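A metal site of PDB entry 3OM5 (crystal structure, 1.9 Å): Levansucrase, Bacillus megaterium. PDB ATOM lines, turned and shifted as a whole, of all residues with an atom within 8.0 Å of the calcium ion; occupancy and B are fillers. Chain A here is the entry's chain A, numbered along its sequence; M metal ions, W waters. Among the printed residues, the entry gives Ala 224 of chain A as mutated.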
ATOM      1  N   GLN A 208      28.057  -3.962   8.320  1.00  0.00           N
ATOM      2  CA  GLN A 208      27.315  -2.747   8.620  1.00  0.00           C
ATOM      3  C   GLN A 208      25.945  -3.037   9.230  1.00  0.00           C
ATOM      4  O   GLN A 208      25.287  -4.007   8.852  1.00  0.00           O
ATOM      5  CB  GLN A 208      27.162  -1.895   7.352  1.00  0.00           C
ATOM      6  CG  GLN A 208      26.670  -0.472   7.607  1.00  0.00           C
ATOM      7  CD  GLN A 208      26.169   0.217   6.348  1.00  0.00           C
ATOM      8  OE1 GLN A 208      25.511  -0.393   5.497  1.00  0.00           O
ATOM      9  NE2 GLN A 208      26.459   1.501   6.239  1.00  0.00           N
ATOM     10  N   PHE A 213      23.892   2.740   8.898  1.00  0.00           N
ATOM     11  CA  PHE A 213      23.296   3.270   7.669  1.00  0.00           C
ATOM     12  C   PHE A 213      22.469   4.527   7.939  1.00  0.00           C
ATOM     13  O   PHE A 213      22.644   5.545   7.263  1.00  0.00           O
ATOM     14  CB  PHE A 213      22.461   2.194   6.960  1.00  0.00           C
ATOM     15  CG  PHE A 213      21.556   2.723   5.872  1.00  0.00           C
ATOM     16  CD1 PHE A 213      22.049   2.992   4.604  1.00  0.00           C
ATOM     17  CD2 PHE A 213      20.196   2.921   6.125  1.00  0.00           C
ATOM     18  CE1 PHE A 213      21.209   3.461   3.604  1.00  0.00           C
ATOM     19  CE2 PHE A 213      19.357   3.400   5.127  1.00  0.00           C
ATOM     20  CZ  PHE A 213      19.864   3.674   3.868  1.00  0.00           C
ATOM     21  N   THR A 221      22.147  10.369   1.252  1.00  0.00           N
ATOM     22  CA  THR A 221      23.384  10.169   0.474  1.00  0.00           C
ATOM     23  C   THR A 221      23.222   9.220  -0.713  1.00  0.00           C
ATOM     24  O   THR A 221      24.020   9.241  -1.659  1.00  0.00           O
ATOM     25  CB  THR A 221      24.522   9.598   1.355  1.00  0.00           C
ATOM     26  OG1 THR A 221      24.119   8.333   1.903  1.00  0.00           O
ATOM     27  CG2 THR A 221      24.881  10.558   2.471  1.00  0.00           C
ATOM     28  N   GLY A 222      22.189   8.383  -0.668  1.00  0.00           N
ATOM     29  CA  GLY A 222      21.985   7.358  -1.686  1.00  0.00           C
ATOM     30  C   GLY A 222      22.706   6.064  -1.360  1.00  0.00           C
ATOM     31  O   GLY A 222      22.918   5.225  -2.233  1.00  0.00           O
ATOM     32  N   ASP A 223      23.088   5.910  -0.093  1.00  0.00           N
ATOM     33  CA  ASP A 223      23.706   4.671   0.387  1.00  0.00           C
ATOM     34  C   ASP A 223      22.699   3.535   0.269  1.00  0.00           C
ATOM     35  O   ASP A 223      21.490   3.760   0.270  1.00  0.00           O
ATOM     36  CB  ASP A 223      24.160   4.822   1.852  1.00  0.00           C
ATOM     37  CG  ASP A 223      25.235   3.824   2.243  1.00  0.00           C
ATOM     38  OD1 ASP A 223      25.994   3.381   1.354  1.00  0.00           O
ATOM     39  OD2 ASP A 223      25.335   3.485   3.439  1.00  0.00           O
ATOM     40  N   ALA A 224      23.196   2.300   0.144  1.00  0.00           N
ATOM     41  CA  ALA A 224      22.322   1.133   0.066  1.00  0.00           C
ATOM     42  C   ALA A 224      22.736   0.081   1.086  1.00  0.00           C
ATOM     43  O   ALA A 224      23.821  -0.507   0.976  1.00  0.00           O
ATOM     44  CB  ALA A 224      22.317   0.566  -1.348  1.00  0.00           C
ATOM     45  N   HIS A 225      21.881  -0.141   2.076  1.00  0.00           N
ATOM     46  CA  HIS A 225      22.153  -1.087   3.147  1.00  0.00           C
ATOM     47  C   HIS A 225      21.596  -2.465   2.829  1.00  0.00           C
ATOM     48  O   HIS A 225      20.417  -2.609   2.477  1.00  0.00           O
ATOM     49  CB  HIS A 225      21.608  -0.587   4.491  1.00  0.00           C
ATOM     50  CG  HIS A 225      21.757  -1.575   5.604  1.00  0.00           C
ATOM     51  ND1 HIS A 225      22.983  -1.988   6.069  1.00  0.00           N
ATOM     52  CD2 HIS A 225      20.832  -2.242   6.339  1.00  0.00           C
ATOM     53  CE1 HIS A 225      22.814  -2.869   7.048  1.00  0.00           C
ATOM     54  NE2 HIS A 225      21.517  -3.039   7.233  1.00  0.00           N
ATOM     55  N   THR A 226      22.443  -3.469   2.985  1.00  0.00           N
ATOM     56  CA  THR A 226      22.070  -4.840   2.645  1.00  0.00           C
ATOM     57  C   THR A 226      22.494  -5.829   3.722  1.00  0.00           C
ATOM     58  O   THR A 226      23.556  -5.665   4.332  1.00  0.00           O
ATOM     59  CB  THR A 226      22.671  -5.287   1.279  1.00  0.00           C
ATOM     60  OG1 THR A 226      24.100  -5.227   1.331  1.00  0.00           O
ATOM     61  CG2 THR A 226      22.203  -4.378   0.142  1.00  0.00           C
ATOM     62  N   ALA A 245      26.111  -8.501   2.088  1.00  0.00           N
ATOM     63  CA  ALA A 245      26.201  -7.496   3.142  1.00  0.00           C
ATOM     64  C   ALA A 245      27.013  -6.283   2.715  1.00  0.00           C
ATOM     65  O   ALA A 245      27.327  -6.098   1.538  1.00  0.00           O
ATOM     66  CB  ALA A 245      26.784  -8.107   4.424  1.00  0.00           C
ATOM     67  N   ASN A 246      27.323  -5.441   3.699  1.00  0.00           N
ATOM     68  CA  ASN A 246      28.196  -4.312   3.489  1.00  0.00           C
ATOM     69  C   ASN A 246      29.248  -4.295   4.581  1.00  0.00           C
ATOM     70  O   ASN A 246      29.004  -4.803   5.681  1.00  0.00           O
ATOM     71  CB  ASN A 246      27.391  -3.022   3.478  1.00  0.00           C
ATOM     72  CG  ASN A 246      26.338  -3.017   2.384  1.00  0.00           C
ATOM     73  OD1 ASN A 246      25.160  -3.297   2.627  1.00  0.00           O
ATOM     74  ND2 ASN A 246      26.759  -2.720   1.154  1.00  0.00           N
ATOM     75  N   THR A 247      30.425  -3.750   4.284  1.00  0.00           N
ATOM     76  CA  THR A 247      31.533  -3.766   5.239  1.00  0.00           C
ATOM     77  C   THR A 247      31.219  -2.996   6.524  1.00  0.00           C
ATOM     78  O   THR A 247      30.415  -2.057   6.509  1.00  0.00           O
ATOM     79  CB  THR A 247      32.857  -3.245   4.625  1.00  0.00           C
ATOM     80  OG1 THR A 247      32.703  -1.874   4.217  1.00  0.00           O
ATOM     81  CG2 THR A 247      33.268  -4.079   3.427  1.00  0.00           C
ATOM     82  N   TYR A 253      35.796   0.179   5.807  1.00  0.00           N
ATOM     83  CA  TYR A 253      34.521   0.881   5.841  1.00  0.00           C
ATOM     84  C   TYR A 253      34.368   1.809   4.660  1.00  0.00           C
ATOM     85  O   TYR A 253      35.361   2.298   4.102  1.00  0.00           O
ATOM     86  CB  TYR A 253      34.349   1.643   7.160  1.00  0.00           C
ATOM     87  CG  TYR A 253      32.910   2.016   7.490  1.00  0.00           C
ATOM     88  CD1 TYR A 253      31.883   1.072   7.411  1.00  0.00           C
ATOM     89  CD2 TYR A 253      32.572   3.313   7.898  1.00  0.00           C
ATOM     90  CE1 TYR A 253      30.575   1.394   7.717  1.00  0.00           C
ATOM     91  CE2 TYR A 253      31.253   3.657   8.206  1.00  0.00           C
ATOM     92  CZ  TYR A 253      30.265   2.691   8.114  1.00  0.00           C
ATOM     93  OH  TYR A 253      28.966   3.014   8.417  1.00  0.00           O
ATOM     94  N   GLN A 254      33.112   2.036   4.280  1.00  0.00           N
ATOM     95  CA  GLN A 254      32.748   3.000   3.251  1.00  0.00           C
ATOM     96  C   GLN A 254      33.238   4.391   3.645  1.00  0.00           C
ATOM     97  O   GLN A 254      33.548   4.643   4.816  1.00  0.00           O
ATOM     98  CB  GLN A 254      31.237   2.995   3.012  1.00  0.00           C
ATOM     99  CG  GLN A 254      30.398   3.407   4.227  1.00  0.00           C
ATOM    100  CD  GLN A 254      28.909   3.293   3.959  1.00  0.00           C
ATOM    101  OE1 GLN A 254      28.439   2.290   3.427  1.00  0.00           O
ATOM    102  NE2 GLN A 254      28.165   4.321   4.333  1.00  0.00           N
ATOM    103  N   GLY A 255      33.321   5.271   2.665  1.00  0.00           N
ATOM    104  CA  GLY A 255      33.802   6.625   2.865  1.00  0.00           C
ATOM    105  C   GLY A 255      34.840   6.990   1.828  1.00  0.00           C
ATOM    106  O   GLY A 255      35.225   6.171   0.988  1.00  0.00           O
ATOM    107  N   GLU A 286      30.718  10.366  -4.791  1.00  0.00           N
ATOM    108  CA  GLU A 286      29.850   9.897  -3.701  1.00  0.00           C
ATOM    109  C   GLU A 286      29.508   8.411  -3.847  1.00  0.00           C
ATOM    110  O   GLU A 286      29.725   7.629  -2.918  1.00  0.00           O
ATOM    111  CB  GLU A 286      28.563  10.719  -3.638  1.00  0.00           C
ATOM    112  CG  GLU A 286      27.586  10.233  -2.582  1.00  0.00           C
ATOM    113  CD  GLU A 286      26.543  11.277  -2.236  1.00  0.00           C
ATOM    114  OE1 GLU A 286      25.586  11.447  -3.015  1.00  0.00           O
ATOM    115  OE2 GLU A 286      26.701  11.930  -1.177  1.00  0.00           O
ATOM    116  N   LYS A 287      28.975   8.046  -5.014  1.00  0.00           N
ATOM    117  CA  LYS A 287      28.575   6.676  -5.285  1.00  0.00           C
ATOM    118  C   LYS A 287      29.705   5.688  -4.945  1.00  0.00           C
ATOM    119  O   LYS A 287      29.498   4.738  -4.208  1.00  0.00           O
ATOM    120  CB  LYS A 287      28.145   6.539  -6.742  1.00  0.00           C
ATOM    121  CG  LYS A 287      27.427   5.255  -7.086  1.00  0.00           C
ATOM    122  CD  LYS A 287      26.989   5.277  -8.533  1.00  0.00           C
ATOM    123  CE  LYS A 287      26.390   3.954  -8.961  1.00  0.00           C
ATOM    124  NZ  LYS A 287      25.973   4.038 -10.380  1.00  0.00           N
ATOM    125  N   ALA A 288      30.903   5.960  -5.474  1.00  0.00           N
ATOM    126  CA  ALA A 288      32.074   5.137  -5.220  1.00  0.00           C
ATOM    127  C   ALA A 288      32.459   5.049  -3.745  1.00  0.00           C
ATOM    128  O   ALA A 288      32.734   3.959  -3.236  1.00  0.00           O
ATOM    129  CB  ALA A 288      33.259   5.640  -6.063  1.00  0.00           C
ATOM    130  N   SER A 289      32.453   6.194  -3.056  1.00  0.00           N
ATOM    131  CA  SER A 289      32.813   6.238  -1.644  1.00  0.00           C
ATOM    132  C   SER A 289      31.878   5.383  -0.798  1.00  0.00           C
ATOM    133  O   SER A 289      32.319   4.689   0.104  1.00  0.00           O
ATOM    134  CB  SER A 289      32.794   7.690  -1.124  1.00  0.00           C
ATOM    135  OG  SER A 289      33.659   8.508  -1.901  1.00  0.00           O
ATOM    136  N   LEU A 290      30.594   5.462  -1.112  1.00  0.00           N
ATOM    137  CA  LEU A 290      29.562   4.722  -0.377  1.00  0.00           C
ATOM    138  C   LEU A 290      29.552   3.242  -0.749  1.00  0.00           C
ATOM    139  O   LEU A 290      29.025   2.427  -0.008  1.00  0.00           O
ATOM    140  CB  LEU A 290      28.178   5.317  -0.664  1.00  0.00           C
ATOM    141  CG  LEU A 290      27.841   6.711  -0.138  1.00  0.00           C
ATOM    142  CD1 LEU A 290      26.516   7.168  -0.753  1.00  0.00           C
ATOM    143  CD2 LEU A 290      27.762   6.696   1.383  1.00  0.00           C
ATOM    144  N   ALA A 291      30.128   2.902  -1.893  1.00  0.00           N
ATOM    145  CA  ALA A 291      30.073   1.524  -2.355  1.00  0.00           C
ATOM    146  C   ALA A 291      30.949   0.629  -1.493  1.00  0.00           C
ATOM    147  O   ALA A 291      32.177   0.721  -1.523  1.00  0.00           O
ATOM    148  CB  ALA A 291      30.469   1.440  -3.830  1.00  0.00           C
ATOM    149  N   ASN A 292      30.309  -0.217  -0.687  1.00  0.00           N
ATOM    150  CA  ASN A 292      31.049  -1.160   0.151  1.00  0.00           C
ATOM    151  C   ASN A 292      30.407  -2.550   0.260  1.00  0.00           C
ATOM    152  O   ASN A 292      30.361  -3.131   1.347  1.00  0.00           O
ATOM    153  CB  ASN A 292      31.356  -0.549   1.547  1.00  0.00           C
ATOM    154  CG  ASN A 292      30.126  -0.398   2.429  1.00  0.00           C
ATOM    155  OD1 ASN A 292      28.989  -0.326   1.964  1.00  0.00           O
ATOM    156  ND2 ASN A 292      30.362  -0.302   3.737  1.00  0.00           N
ATOM    157  N   GLY A 293      29.935  -3.066  -0.864  1.00  0.00           N
ATOM    158  CA  GLY A 293      29.361  -4.418  -0.914  1.00  0.00           C
ATOM    159  C   GLY A 293      30.336  -5.474  -0.416  1.00  0.00           C
ATOM    160  O   GLY A 293      31.549  -5.336  -0.570  1.00  0.00           O
ATOM    161  N   ASN A 317      34.332  -2.860  -2.577  1.00  0.00           N
ATOM    162  CA  ASN A 317      34.507  -1.437  -2.222  1.00  0.00           C
ATOM    163  C   ASN A 317      34.834  -0.602  -3.462  1.00  0.00           C
ATOM    164  O   ASN A 317      35.649  -1.009  -4.289  1.00  0.00           O
ATOM    165  CB  ASN A 317      35.645  -1.253  -1.210  1.00  0.00           C
ATOM    166  CG  ASN A 317      35.282  -1.696   0.201  1.00  0.00           C
ATOM    167  OD1 ASN A 317      35.238  -2.900   0.512  1.00  0.00           O
ATOM    168  ND2 ASN A 317      35.075  -0.725   1.092  1.00  0.00           N
ATOM    169  N   THR A 320      30.777  -1.404  -6.195  1.00  0.00           N
ATOM    170  CA  THR A 320      29.319  -1.384  -6.010  1.00  0.00           C
ATOM    171  C   THR A 320      28.926  -1.622  -4.563  1.00  0.00           C
ATOM    172  O   THR A 320      29.687  -2.178  -3.772  1.00  0.00           O
ATOM    173  CB  THR A 320      28.589  -2.392  -6.948  1.00  0.00           C
ATOM    174  OG1 THR A 320      27.171  -2.362  -6.683  1.00  0.00           O
ATOM    175  CG2 THR A 320      29.123  -3.798  -6.755  1.00  0.00           C
ATOM    176  N   ASP A 321      27.705  -1.207  -4.218  1.00  0.00           N
ATOM    177  CA  ASP A 321      27.198  -1.352  -2.873  1.00  0.00           C
ATOM    178  C   ASP A 321      26.321  -2.597  -2.788  1.00  0.00           C
ATOM    179  O   ASP A 321      25.817  -2.953  -1.722  1.00  0.00           O
ATOM    180  CB  ASP A 321      26.414  -0.109  -2.488  1.00  0.00           C
ATOM    181  CG  ASP A 321      26.611   0.286  -1.046  1.00  0.00           C
ATOM    182  OD1 ASP A 321      27.427  -0.343  -0.340  1.00  0.00           O
ATOM    183  OD2 ASP A 321      25.958   1.258  -0.603  1.00  0.00           O
ATOM    184  N   GLU A 322      26.160  -3.259  -3.940  1.00  0.00           N
ATOM    185  CA  GLU A 322      25.230  -4.375  -4.079  1.00  0.00           C
ATOM    186  C   GLU A 322      25.790  -5.548  -4.888  1.00  0.00           C
ATOM    187  O   GLU A 322      25.831  -5.515  -6.112  1.00  0.00           O
ATOM    188  CB  GLU A 322      23.886  -3.897  -4.657  1.00  0.00           C
ATOM    189  CG  GLU A 322      23.200  -2.826  -3.818  1.00  0.00           C
ATOM    190  CD  GLU A 322      21.714  -2.700  -4.072  1.00  0.00           C
ATOM    191  OE1 GLU A 322      21.235  -1.554  -4.185  1.00  0.00           O
ATOM    192  OE2 GLU A 322      21.027  -3.737  -4.158  1.00  0.00           O
HETATM  193 CA    CA M   1      27.569   1.477   1.352  1.00  0.00          CA
HETATM  194  O   HOH W   1      26.133  -0.131   2.841  1.00  0.00           O
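Water W1 lies within hydrogen-bond range of the side-chain amide oxygen of Gln 208 (2.7 Å), the backbone carbonyl oxygen of Ala 224 (3.0 Å) and the side-chain amide nitrogen of Asn 246 (3.2 Å).
Five residues have an atom within 4 Å of the calcium ion: Asp 223, Gln 254, Leu 290, Asn 292 and Asp 321. The nearest printed residue that does not touch the calcium ion is Ala 224 (4.3 Å).
O of Leu 290 is bound to the calcium ion (2.2 Å). OD1 of Asn 292 binds the calcium ion (2.4 Å). The calcium ion is bound by OE1 of Gln 254. The side-chain carboxylate (OD1) of Asp 223 binds the calcium ion (2.5 Å). The calcium ion is bound by the side-chain carboxylate (OD1) of Asp 321, 2.5 Å away. OD2 of Asp 321 is bound to the calcium ion, 2.5 Å away. Water W1 is bound to the calcium ion (2.6 Å).
The backbone carbonyl oxygen (O) of Asp 321 sits at hydrogen-bond distance from the side-chain amide nitrogen (ND2) of Asn 246. OG1 of Thr 221 lies within hydrogen-bond range of N of Asp 223 (3.3 Å). OD1 of Asn 292 lies close to ND2 of Asn 246, 3.4 Å away. OG1 of Thr 247 sits at hydrogen-bond distance from ND2 of Asn 292 (2.9 Å). OD2 of Asp 321 sits close to N of Ala 224, 3.0 Å away.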
